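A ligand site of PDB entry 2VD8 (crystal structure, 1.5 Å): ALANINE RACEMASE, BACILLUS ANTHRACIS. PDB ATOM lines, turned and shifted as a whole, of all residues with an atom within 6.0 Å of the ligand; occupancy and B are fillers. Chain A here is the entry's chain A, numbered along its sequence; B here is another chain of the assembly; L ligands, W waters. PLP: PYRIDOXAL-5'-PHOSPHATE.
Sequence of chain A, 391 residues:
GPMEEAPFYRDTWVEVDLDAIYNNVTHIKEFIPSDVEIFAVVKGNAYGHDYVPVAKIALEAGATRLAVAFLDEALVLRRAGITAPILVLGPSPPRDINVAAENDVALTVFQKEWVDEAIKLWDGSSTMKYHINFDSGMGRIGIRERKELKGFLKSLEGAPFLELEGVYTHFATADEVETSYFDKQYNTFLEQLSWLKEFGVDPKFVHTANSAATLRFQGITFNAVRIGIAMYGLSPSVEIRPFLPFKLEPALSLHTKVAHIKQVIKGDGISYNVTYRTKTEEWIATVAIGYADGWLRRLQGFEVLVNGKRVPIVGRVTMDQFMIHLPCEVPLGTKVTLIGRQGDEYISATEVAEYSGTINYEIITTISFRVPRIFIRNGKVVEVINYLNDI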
ATOM      1  N   VAL A  41     -13.071  22.141  17.621  1.00  0.00           N
ATOM      2  CA  VAL A  41     -14.485  21.891  17.374  1.00  0.00           C
ATOM      3  C   VAL A  41     -15.320  22.777  18.296  1.00  0.00           C
ATOM      4  O   VAL A  41     -15.300  22.590  19.515  1.00  0.00           O
ATOM      5  CB  VAL A  41     -14.856  20.435  17.605  1.00  0.00           C
ATOM      6  CG1 VAL A  41     -16.319  20.217  17.334  1.00  0.00           C
ATOM      7  CG2 VAL A  41     -13.990  19.527  16.687  1.00  0.00           C
ATOM      8  N   LYS A  43     -18.758  23.536  17.745  1.00  0.00           N
ATOM      9  CA  LYS A  43     -20.201  23.312  17.640  1.00  0.00           C
ATOM     10  C   LYS A  43     -20.875  23.502  19.001  1.00  0.00           C
ATOM     11  O   LYS A  43     -20.227  23.433  20.068  1.00  0.00           O
ATOM     12  CB  LYS A  43     -20.498  21.936  17.077  1.00  0.00           C
ATOM     13  CG  LYS A  43     -20.094  20.818  17.982  1.00  0.00           C
ATOM     14  CD  LYS A  43     -20.050  19.449  17.280  1.00  0.00           C
ATOM     15  CE  LYS A  43     -19.461  18.404  18.257  1.00  0.00           C
ATOM     16  NZ  LYS A  43     -19.546  16.971  17.845  1.00  0.00           N
ATOM     17  N   TYR A  47     -19.457  24.294  22.874  1.00  0.00           N
ATOM     18  CA  TYR A  47     -19.775  23.441  24.039  1.00  0.00           C
ATOM     19  C   TYR A  47     -20.118  24.310  25.243  1.00  0.00           C
ATOM     20  O   TYR A  47     -19.716  24.036  26.396  1.00  0.00           O
ATOM     21  CB  TYR A  47     -18.610  22.508  24.402  1.00  0.00           C
ATOM     22  CG  TYR A  47     -18.319  21.381  23.421  1.00  0.00           C
ATOM     23  CD1 TYR A  47     -18.275  21.573  22.037  1.00  0.00           C
ATOM     24  CD2 TYR A  47     -17.964  20.116  23.886  1.00  0.00           C
ATOM     25  CE1 TYR A  47     -17.940  20.527  21.156  1.00  0.00           C
ATOM     26  CE2 TYR A  47     -17.630  19.053  23.017  1.00  0.00           C
ATOM     27  CZ  TYR A  47     -17.612  19.255  21.664  1.00  0.00           C
ATOM     28  OH  TYR A  47     -17.298  18.208  20.833  1.00  0.00           O
ATOM     29  N   LEU A  89     -19.671  19.893  10.198  1.00  0.00           N
ATOM     30  CA  LEU A  89     -19.608  18.444  10.447  1.00  0.00           C
ATOM     31  C   LEU A  89     -20.937  17.742  10.271  1.00  0.00           C
ATOM     32  O   LEU A  89     -20.993  16.578   9.860  1.00  0.00           O
ATOM     33  CB  LEU A  89     -19.097  18.155  11.859  1.00  0.00           C
ATOM     34  CG  LEU A  89     -17.650  18.560  12.136  1.00  0.00           C
ATOM     35  CD1 LEU A  89     -17.349  18.486  13.644  1.00  0.00           C
ATOM     36  CD2 LEU A  89     -16.688  17.692  11.330  1.00  0.00           C
ATOM     37  N   ASN A 133     -17.728  12.445   4.367  1.00  0.00           N
ATOM     38  CA  ASN A 133     -17.822  11.692   5.610  1.00  0.00           C
ATOM     39  C   ASN A 133     -18.051  10.256   5.208  1.00  0.00           C
ATOM     40  O   ASN A 133     -19.015   9.965   4.473  1.00  0.00           O
ATOM     41  CB  ASN A 133     -18.984  12.228   6.460  1.00  0.00           C
ATOM     42  CG  ASN A 133     -19.159  11.501   7.757  1.00  0.00           C
ATOM     43  OD1 ASN A 133     -18.955  10.273   7.835  1.00  0.00           O
ATOM     44  ND2 ASN A 133     -19.583  12.233   8.797  1.00  0.00           N
ATOM     45  N   ARG A 140     -24.399   7.501  11.815  1.00  0.00           N
ATOM     46  CA  ARG A 140     -25.074   8.806  11.889  1.00  0.00           C
ATOM     47  C   ARG A 140     -25.261   9.397  10.495  1.00  0.00           C
ATOM     48  O   ARG A 140     -26.356   9.311   9.914  1.00  0.00           O
ATOM     49  CB  ARG A 140     -24.300   9.742  12.843  1.00  0.00           C
ATOM     50  CG  ARG A 140     -24.853  11.147  13.011  1.00  0.00           C
ATOM     51  CD  ARG A 140     -24.236  11.824  14.221  1.00  0.00           C
ATOM     52  NE  ARG A 140     -22.800  12.044  14.110  1.00  0.00           N
ATOM     53  CZ  ARG A 140     -22.090  12.741  15.000  1.00  0.00           C
ATOM     54  NH1 ARG A 140     -22.681  13.290  16.057  1.00  0.00           N
ATOM     55  NH2 ARG A 140     -20.771  12.885  14.849  1.00  0.00           N
ATOM     56  N   TYR A 168     -13.134  12.051   5.988  1.00  0.00           N
ATOM     57  CA  TYR A 168     -13.105  11.783   7.405  1.00  0.00           C
ATOM     58  C   TYR A 168     -14.048  10.698   7.824  1.00  0.00           C
ATOM     59  O   TYR A 168     -14.972  10.348   7.095  1.00  0.00           O
ATOM     60  CB  TYR A 168     -13.321  13.085   8.200  1.00  0.00           C
ATOM     61  CG  TYR A 168     -14.745  13.587   8.315  1.00  0.00           C
ATOM     62  CD1 TYR A 168     -15.298  14.442   7.346  1.00  0.00           C
ATOM     63  CD2 TYR A 168     -15.517  13.270   9.436  1.00  0.00           C
ATOM     64  CE1 TYR A 168     -16.575  14.928   7.493  1.00  0.00           C
ATOM     65  CE2 TYR A 168     -16.799  13.750   9.576  1.00  0.00           C
ATOM     66  CZ  TYR A 168     -17.337  14.591   8.604  1.00  0.00           C
ATOM     67  OH  TYR A 168     -18.643  15.062   8.711  1.00  0.00           O
ATOM     68  N   THR A 169     -13.792  10.162   9.001  1.00  0.00           N
ATOM     69  CA  THR A 169     -14.758   9.326   9.705  1.00  0.00           C
ATOM     70  C   THR A 169     -14.756   9.740  11.173  1.00  0.00           C
ATOM     71  O   THR A 169     -13.980  10.606  11.573  1.00  0.00           O
ATOM     72  CB  THR A 169     -14.479   7.792   9.522  1.00  0.00           C
ATOM     73  OG1 THR A 169     -15.629   7.026   9.906  1.00  0.00           O
ATOM     74  CG2 THR A 169     -13.265   7.326  10.346  1.00  0.00           C
ATOM     75  N   HIS A 170     -15.630   9.111  11.968  1.00  0.00           N
ATOM     76  CA  HIS A 170     -15.819   9.423  13.373  1.00  0.00           C
ATOM     77  C   HIS A 170     -16.023   8.116  14.135  1.00  0.00           C
ATOM     78  O   HIS A 170     -16.717   7.216  13.670  1.00  0.00           O
ATOM     79  CB  HIS A 170     -17.034  10.324  13.556  1.00  0.00           C
ATOM     80  CG  HIS A 170     -17.170  10.935  14.920  1.00  0.00           C
ATOM     81  ND1 HIS A 170     -16.210  11.759  15.473  1.00  0.00           N
ATOM     82  CD2 HIS A 170     -18.176  10.853  15.831  1.00  0.00           C
ATOM     83  CE1 HIS A 170     -16.629  12.163  16.673  1.00  0.00           C
ATOM     84  NE2 HIS A 170     -17.806  11.616  16.915  1.00  0.00           N
ATOM     85  N   ALA A 209      -9.883  11.379  14.195  1.00  0.00           N
ATOM     86  CA  ALA A 209      -9.835  11.240  15.656  1.00  0.00           C
ATOM     87  C   ALA A 209     -10.489  12.399  16.396  1.00  0.00           C
ATOM     88  O   ALA A 209     -10.152  13.565  16.169  1.00  0.00           O
ATOM     89  CB  ALA A 209      -8.384  11.105  16.120  1.00  0.00           C
ATOM     90  N   ASN A 210     -11.401  12.046  17.306  1.00  0.00           N
ATOM     91  CA  ASN A 210     -11.942  12.968  18.303  1.00  0.00           C
ATOM     92  C   ASN A 210     -10.982  13.072  19.500  1.00  0.00           C
ATOM     93  O   ASN A 210      -9.853  12.603  19.427  1.00  0.00           O
ATOM     94  CB  ASN A 210     -13.354  12.533  18.736  1.00  0.00           C
ATOM     95  CG  ASN A 210     -13.400  11.108  19.244  1.00  0.00           C
ATOM     96  OD1 ASN A 210     -12.357  10.461  19.384  1.00  0.00           O
ATOM     97  ND2 ASN A 210     -14.617  10.603  19.493  1.00  0.00           N
ATOM     98  N   SER A 211     -11.405  13.721  20.581  1.00  0.00           N
ATOM     99  CA  SER A 211     -10.515  13.835  21.757  1.00  0.00           C
ATOM    100  C   SER A 211     -10.051  12.468  22.271  1.00  0.00           C
ATOM    101  O   SER A 211      -8.856  12.258  22.501  1.00  0.00           O
ATOM    102  CB  SER A 211     -11.209  14.552  22.895  1.00  0.00           C
ATOM    103  OG  SER A 211     -11.485  15.902  22.587  1.00  0.00           O
ATOM    104  N   ALA A 212     -10.995  11.551  22.442  1.00  0.00           N
ATOM    105  CA  ALA A 212     -10.684  10.266  23.035  1.00  0.00           C
ATOM    106  C   ALA A 212      -9.686   9.495  22.160  1.00  0.00           C
ATOM    107  O   ALA A 212      -8.645   9.003  22.645  1.00  0.00           O
ATOM    108  CB  ALA A 212     -11.940   9.471  23.217  1.00  0.00           C
ATOM    109  N   ARG A 226      -9.707  16.194  15.367  1.00  0.00           N
ATOM    110  CA  ARG A 226     -10.851  17.072  15.623  1.00  0.00           C
ATOM    111  C   ARG A 226     -11.128  17.065  17.130  1.00  0.00           C
ATOM    112  O   ARG A 226     -11.669  16.112  17.675  1.00  0.00           O
ATOM    113  CB  ARG A 226     -12.100  16.585  14.883  1.00  0.00           C
ATOM    114  CG  ARG A 226     -11.975  16.529  13.373  1.00  0.00           C
ATOM    115  CD  ARG A 226     -13.301  16.265  12.654  1.00  0.00           C
ATOM    116  NE  ARG A 226     -13.933  15.038  13.138  1.00  0.00           N
ATOM    117  CZ  ARG A 226     -13.588  13.808  12.763  1.00  0.00           C
ATOM    118  NH1 ARG A 226     -12.658  13.598  11.850  1.00  0.00           N
ATOM    119  NH2 ARG A 226     -14.197  12.776  13.333  1.00  0.00           N
ATOM    120  N   ILE A 227     -10.713  18.128  17.804  1.00  0.00           N
ATOM    121  CA  ILE A 227     -10.787  18.195  19.246  1.00  0.00           C
ATOM    122  C   ILE A 227     -11.911  19.074  19.767  1.00  0.00           C
ATOM    123  O   ILE A 227     -11.932  20.277  19.515  1.00  0.00           O
ATOM    124  CB  ILE A 227      -9.463  18.721  19.833  1.00  0.00           C
ATOM    125  CG1 ILE A 227      -8.270  17.963  19.258  1.00  0.00           C
ATOM    126  CG2 ILE A 227      -9.503  18.681  21.348  1.00  0.00           C
ATOM    127  CD1 ILE A 227      -8.224  16.463  19.662  1.00  0.00           C
ATOM    128  N   GLY A 228     -12.829  18.471  20.510  1.00  0.00           N
ATOM    129  CA  GLY A 228     -13.861  19.189  21.240  1.00  0.00           C
ATOM    130  C   GLY A 228     -13.569  19.115  22.712  1.00  0.00           C
ATOM    131  O   GLY A 228     -12.848  19.965  23.262  1.00  0.00           O
ATOM    132  N   ILE A 229     -14.120  18.095  23.372  1.00  0.00           N
ATOM    133  CA  ILE A 229     -14.172  18.025  24.844  1.00  0.00           C
ATOM    134  C   ILE A 229     -12.811  18.260  25.538  1.00  0.00           C
ATOM    135  O   ILE A 229     -12.730  19.008  26.542  1.00  0.00           O
ATOM    136  CB  ILE A 229     -14.880  16.710  25.305  1.00  0.00           C
ATOM    137  CG1 ILE A 229     -15.387  16.824  26.752  1.00  0.00           C
ATOM    138  CG2 ILE A 229     -13.993  15.500  25.144  1.00  0.00           C
ATOM    139  CD1 ILE A 229     -16.574  17.768  26.910  1.00  0.00           C
ATOM    140  N   ALA A 230     -11.733  17.684  25.014  1.00  0.00           N
ATOM    141  CA  ALA A 230     -10.415  17.833  25.655  1.00  0.00           C
ATOM    142  C   ALA A 230      -9.908  19.275  25.582  1.00  0.00           C
ATOM    143  O   ALA A 230      -9.203  19.722  26.499  1.00  0.00           O
ATOM    144  CB  ALA A 230      -9.418  16.878  25.057  1.00  0.00           C
ATOM    145  N   PRO A 236     -13.365  12.820  27.868  1.00  0.00           N
ATOM    146  CA  PRO A 236     -14.432  12.253  27.053  1.00  0.00           C
ATOM    147  C   PRO A 236     -15.367  11.296  27.812  1.00  0.00           C
ATOM    148  O   PRO A 236     -16.561  11.235  27.527  1.00  0.00           O
ATOM    149  CB  PRO A 236     -13.682  11.532  25.928  1.00  0.00           C
ATOM    150  CG  PRO A 236     -12.418  12.287  25.811  1.00  0.00           C
ATOM    151  CD  PRO A 236     -12.048  12.706  27.206  1.00  0.00           C
ATOM    152  N   TYR A 361     -20.715  16.594  28.363  1.00  0.00           N
ATOM    153  CA  TYR A 361     -20.991  17.316  27.121  1.00  0.00           C
ATOM    154  C   TYR A 361     -22.347  18.017  27.190  1.00  0.00           C
ATOM    155  O   TYR A 361     -22.496  19.139  26.716  1.00  0.00           O
ATOM    156  CB  TYR A 361     -21.095  16.374  25.926  1.00  0.00           C
ATOM    157  CG  TYR A 361     -19.844  15.649  25.487  1.00  0.00           C
ATOM    158  CD1 TYR A 361     -19.364  14.541  26.199  1.00  0.00           C
ATOM    159  CD2 TYR A 361     -19.184  15.989  24.328  1.00  0.00           C
ATOM    160  CE1 TYR A 361     -18.264  13.861  25.787  1.00  0.00           C
ATOM    161  CE2 TYR A 361     -18.079  15.293  23.893  1.00  0.00           C
ATOM    162  CZ  TYR A 361     -17.622  14.233  24.637  1.00  0.00           C
ATOM    163  OH  TYR A 361     -16.495  13.551  24.188  1.00  0.00           O
ATOM    164  N   TYR B 272     -23.237   6.630  19.450  1.00  0.00           N
ATOM    165  CA  TYR B 272     -22.184   6.446  20.448  1.00  0.00           C
ATOM    166  C   TYR B 272     -22.458   5.219  21.306  1.00  0.00           C
ATOM    167  O   TYR B 272     -23.606   4.961  21.683  1.00  0.00           O
ATOM    168  CB  TYR B 272     -22.063   7.668  21.346  1.00  0.00           C
ATOM    169  CG  TYR B 272     -21.428   8.875  20.694  1.00  0.00           C
ATOM    170  CD1 TYR B 272     -20.117   8.843  20.236  1.00  0.00           C
ATOM    171  CD2 TYR B 272     -22.133  10.063  20.529  1.00  0.00           C
ATOM    172  CE1 TYR B 272     -19.527   9.928  19.617  1.00  0.00           C
ATOM    173  CE2 TYR B 272     -21.550  11.167  19.904  1.00  0.00           C
ATOM    174  CZ  TYR B 272     -20.246  11.089  19.468  1.00  0.00           C
ATOM    175  OH  TYR B 272     -19.658  12.190  18.855  1.00  0.00           O
ATOM    176  N   MET B 319     -24.892  15.682  19.809  1.00  0.00           N
ATOM    177  CA  MET B 319     -24.986  17.104  20.115  1.00  0.00           C
ATOM    178  C   MET B 319     -25.902  17.824  19.154  1.00  0.00           C
ATOM    179  O   MET B 319     -26.639  18.726  19.559  1.00  0.00           O
ATOM    180  CB  MET B 319     -23.618  17.802  20.110  1.00  0.00           C
ATOM    181  CG  MET B 319     -23.638  19.234  20.660  1.00  0.00           C
ATOM    182  SD  MET B 319     -22.002  19.945  20.889  1.00  0.00           S
ATOM    183  CE  MET B 319     -21.458  19.019  22.334  1.00  0.00           C
ATOM    184  N   ASP B 320     -25.840  17.419  17.893  1.00  0.00           N
ATOM    185  CA  ASP B 320     -26.497  18.144  16.822  1.00  0.00           C
ATOM    186  C   ASP B 320     -27.376  17.277  15.912  1.00  0.00           C
ATOM    187  O   ASP B 320     -27.918  17.790  14.959  1.00  0.00           O
ATOM    188  CB  ASP B 320     -25.440  18.824  15.965  1.00  0.00           C
ATOM    189  CG  ASP B 320     -24.352  19.458  16.789  1.00  0.00           C
ATOM    190  OD1 ASP B 320     -24.609  20.457  17.500  1.00  0.00           O
ATOM    191  OD2 ASP B 320     -23.212  18.953  16.717  1.00  0.00           O
ATOM    192  N   GLN B 321     -27.490  15.986  16.209  1.00  0.00           N
ATOM    193  CA  GLN B 321     -28.181  15.044  15.335  1.00  0.00           C
ATOM    194  C   GLN B 321     -28.735  13.889  16.151  1.00  0.00           C
ATOM    195  O   GLN B 321     -28.195  13.528  17.181  1.00  0.00           O
ATOM    196  CB  GLN B 321     -27.220  14.443  14.317  1.00  0.00           C
ATOM    197  CG  GLN B 321     -26.467  15.438  13.451  1.00  0.00           C
ATOM    198  CD  GLN B 321     -25.412  14.767  12.579  1.00  0.00           C
ATOM    199  OE1 GLN B 321     -25.741  13.986  11.681  1.00  0.00           O
ATOM    200  NE2 GLN B 321     -24.147  15.087  12.818  1.00  0.00           N
HETATM  201  N1  PLP L   1     -15.881  15.100  15.199  1.00  0.00           N
HETATM  202  C2  PLP L   1     -17.255  14.992  14.999  1.00  0.00           C
HETATM  203  C2A PLP L   1     -17.750  14.517  13.663  1.00  0.00           C
HETATM  204  C3  PLP L   1     -18.127  15.354  16.027  1.00  0.00           C
HETATM  205  O3  PLP L   1     -19.379  15.268  15.915  1.00  0.00           O
HETATM  206  C4  PLP L   1     -17.586  15.800  17.253  1.00  0.00           C
HETATM  207  C4A PLP L   1     -18.535  16.194  18.358  1.00  0.00           C
HETATM  208  C5  PLP L   1     -16.201  15.905  17.431  1.00  0.00           C
HETATM  209  C6  PLP L   1     -15.349  15.537  16.395  1.00  0.00           C
HETATM  210  C5A PLP L   1     -15.612  16.306  18.750  1.00  0.00           C
HETATM  211  O4P PLP L   1     -15.681  15.194  19.708  1.00  0.00           O
HETATM  212  P   PLP L   1     -15.035  15.321  21.195  1.00  0.00           P
HETATM  213  O1P PLP L   1     -15.316  14.032  21.877  1.00  0.00           O
HETATM  214  O2P PLP L   1     -13.595  15.508  20.967  1.00  0.00           O
HETATM  215  O3P PLP L   1     -15.717  16.502  21.809  1.00  0.00           O
HETATM  216  O   HOH W   1     -13.805  11.923  22.397  1.00  0.00           O
HETATM  217  O   HOH W   2     -21.126  16.121  13.991  1.00  0.00           O
HETATM  218  O   HOH W   3     -16.928  12.209  20.246  1.00  0.00           O
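The side-chain amino group (NZ) of Lys 43 is covalently linked to a carbon (C4A) of the ligand (1.4 Å).
OH of Tyr 47 sits at hydrogen-bond distance from O3P of the ligand (2.5 Å).
An oxygen (O1P) of the ligand sits at hydrogen-bond distance from the side-chain hydroxyl (OH) of Tyr 361, 2.6 Å away.
N of Ser 211 sits at hydrogen-bond distance from O2P of the ligand (2.9 Å).
OG of Ser 211 lies within hydrogen-bond range of O2P of the ligand (2.7 Å).
N of Ile 229 sits at hydrogen-bond distance from O3P of the ligand (2.7 Å).
N1 of the ligand is in hydrogen-bond range of NE of Arg 226.
O3 of the ligand sits at hydrogen-bond distance from NH2 of Arg 140.
The backbone NH (N) of Gly 228 is in hydrogen-bond range of an oxygen (O2P) of the ligand (3.1 Å).
A ring nitrogen (ND1) of His 170 is in hydrogen-bond range of a nitrogen (N1) of the ligand (3.4 Å).
Merely in contact with the ligand: Leu 89 and Asn 210.
Hydrophobic or aromatic side chains that line the ligand: Tyr 47, Leu 89, His 170, Ile 229 and Tyr 361.
11 residues have an atom within 4 Å of the ligand: Lys 43, Tyr 47, Leu 89, Arg 140, His 170, Asn 210, Ser 211, Arg 226, Gly 228, Ile 229 and Tyr 361.
The nearest printed residue that does not touch the ligand is Ile 227 (4.1 Å).
The backbone NH (N) of Ala 230 is in hydrogen-bond range of the side-chain hydroxyl (OG) of Ser 211 (3.0 Å).
The guanidinium group of Arg 226 sits at hydrogen-bond distance from a ring nitrogen (ND1) of His 170.
N of Arg 226 sits at hydrogen-bond distance from O of Ala 209 (2.8 Å).
NH2 of Arg 226 lies within hydrogen-bond range of O of Thr 169, 2.8 Å away.
OH of Tyr 272 of chain B sits at hydrogen-bond distance from NE2 of His 170 (2.7 Å).
O of Leu 89 is in hydrogen-bond range of OH of Tyr 168.
Water W1 lies within hydrogen-bond range of an oxygen (O1P) of the ligand, the backbone NH (N) of Ala 212 and the side-chain amide nitrogen (ND2) of Asn 210.
Water W2 lies within hydrogen-bond range of O3 of the ligand, NH2 of Arg 140 and NE2 of Gln 321 of chain B.
Water W3 lies within hydrogen-bond range of the side-chain amide nitrogen (ND2) of Asn 210 (2.9 Å), an oxygen (O1P) of the ligand (2.9 Å), the side-chain hydroxyl (OH) of Tyr 272 of chain B (3.1 Å) and a ring nitrogen (NE2) of His 170 (3.5 Å).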
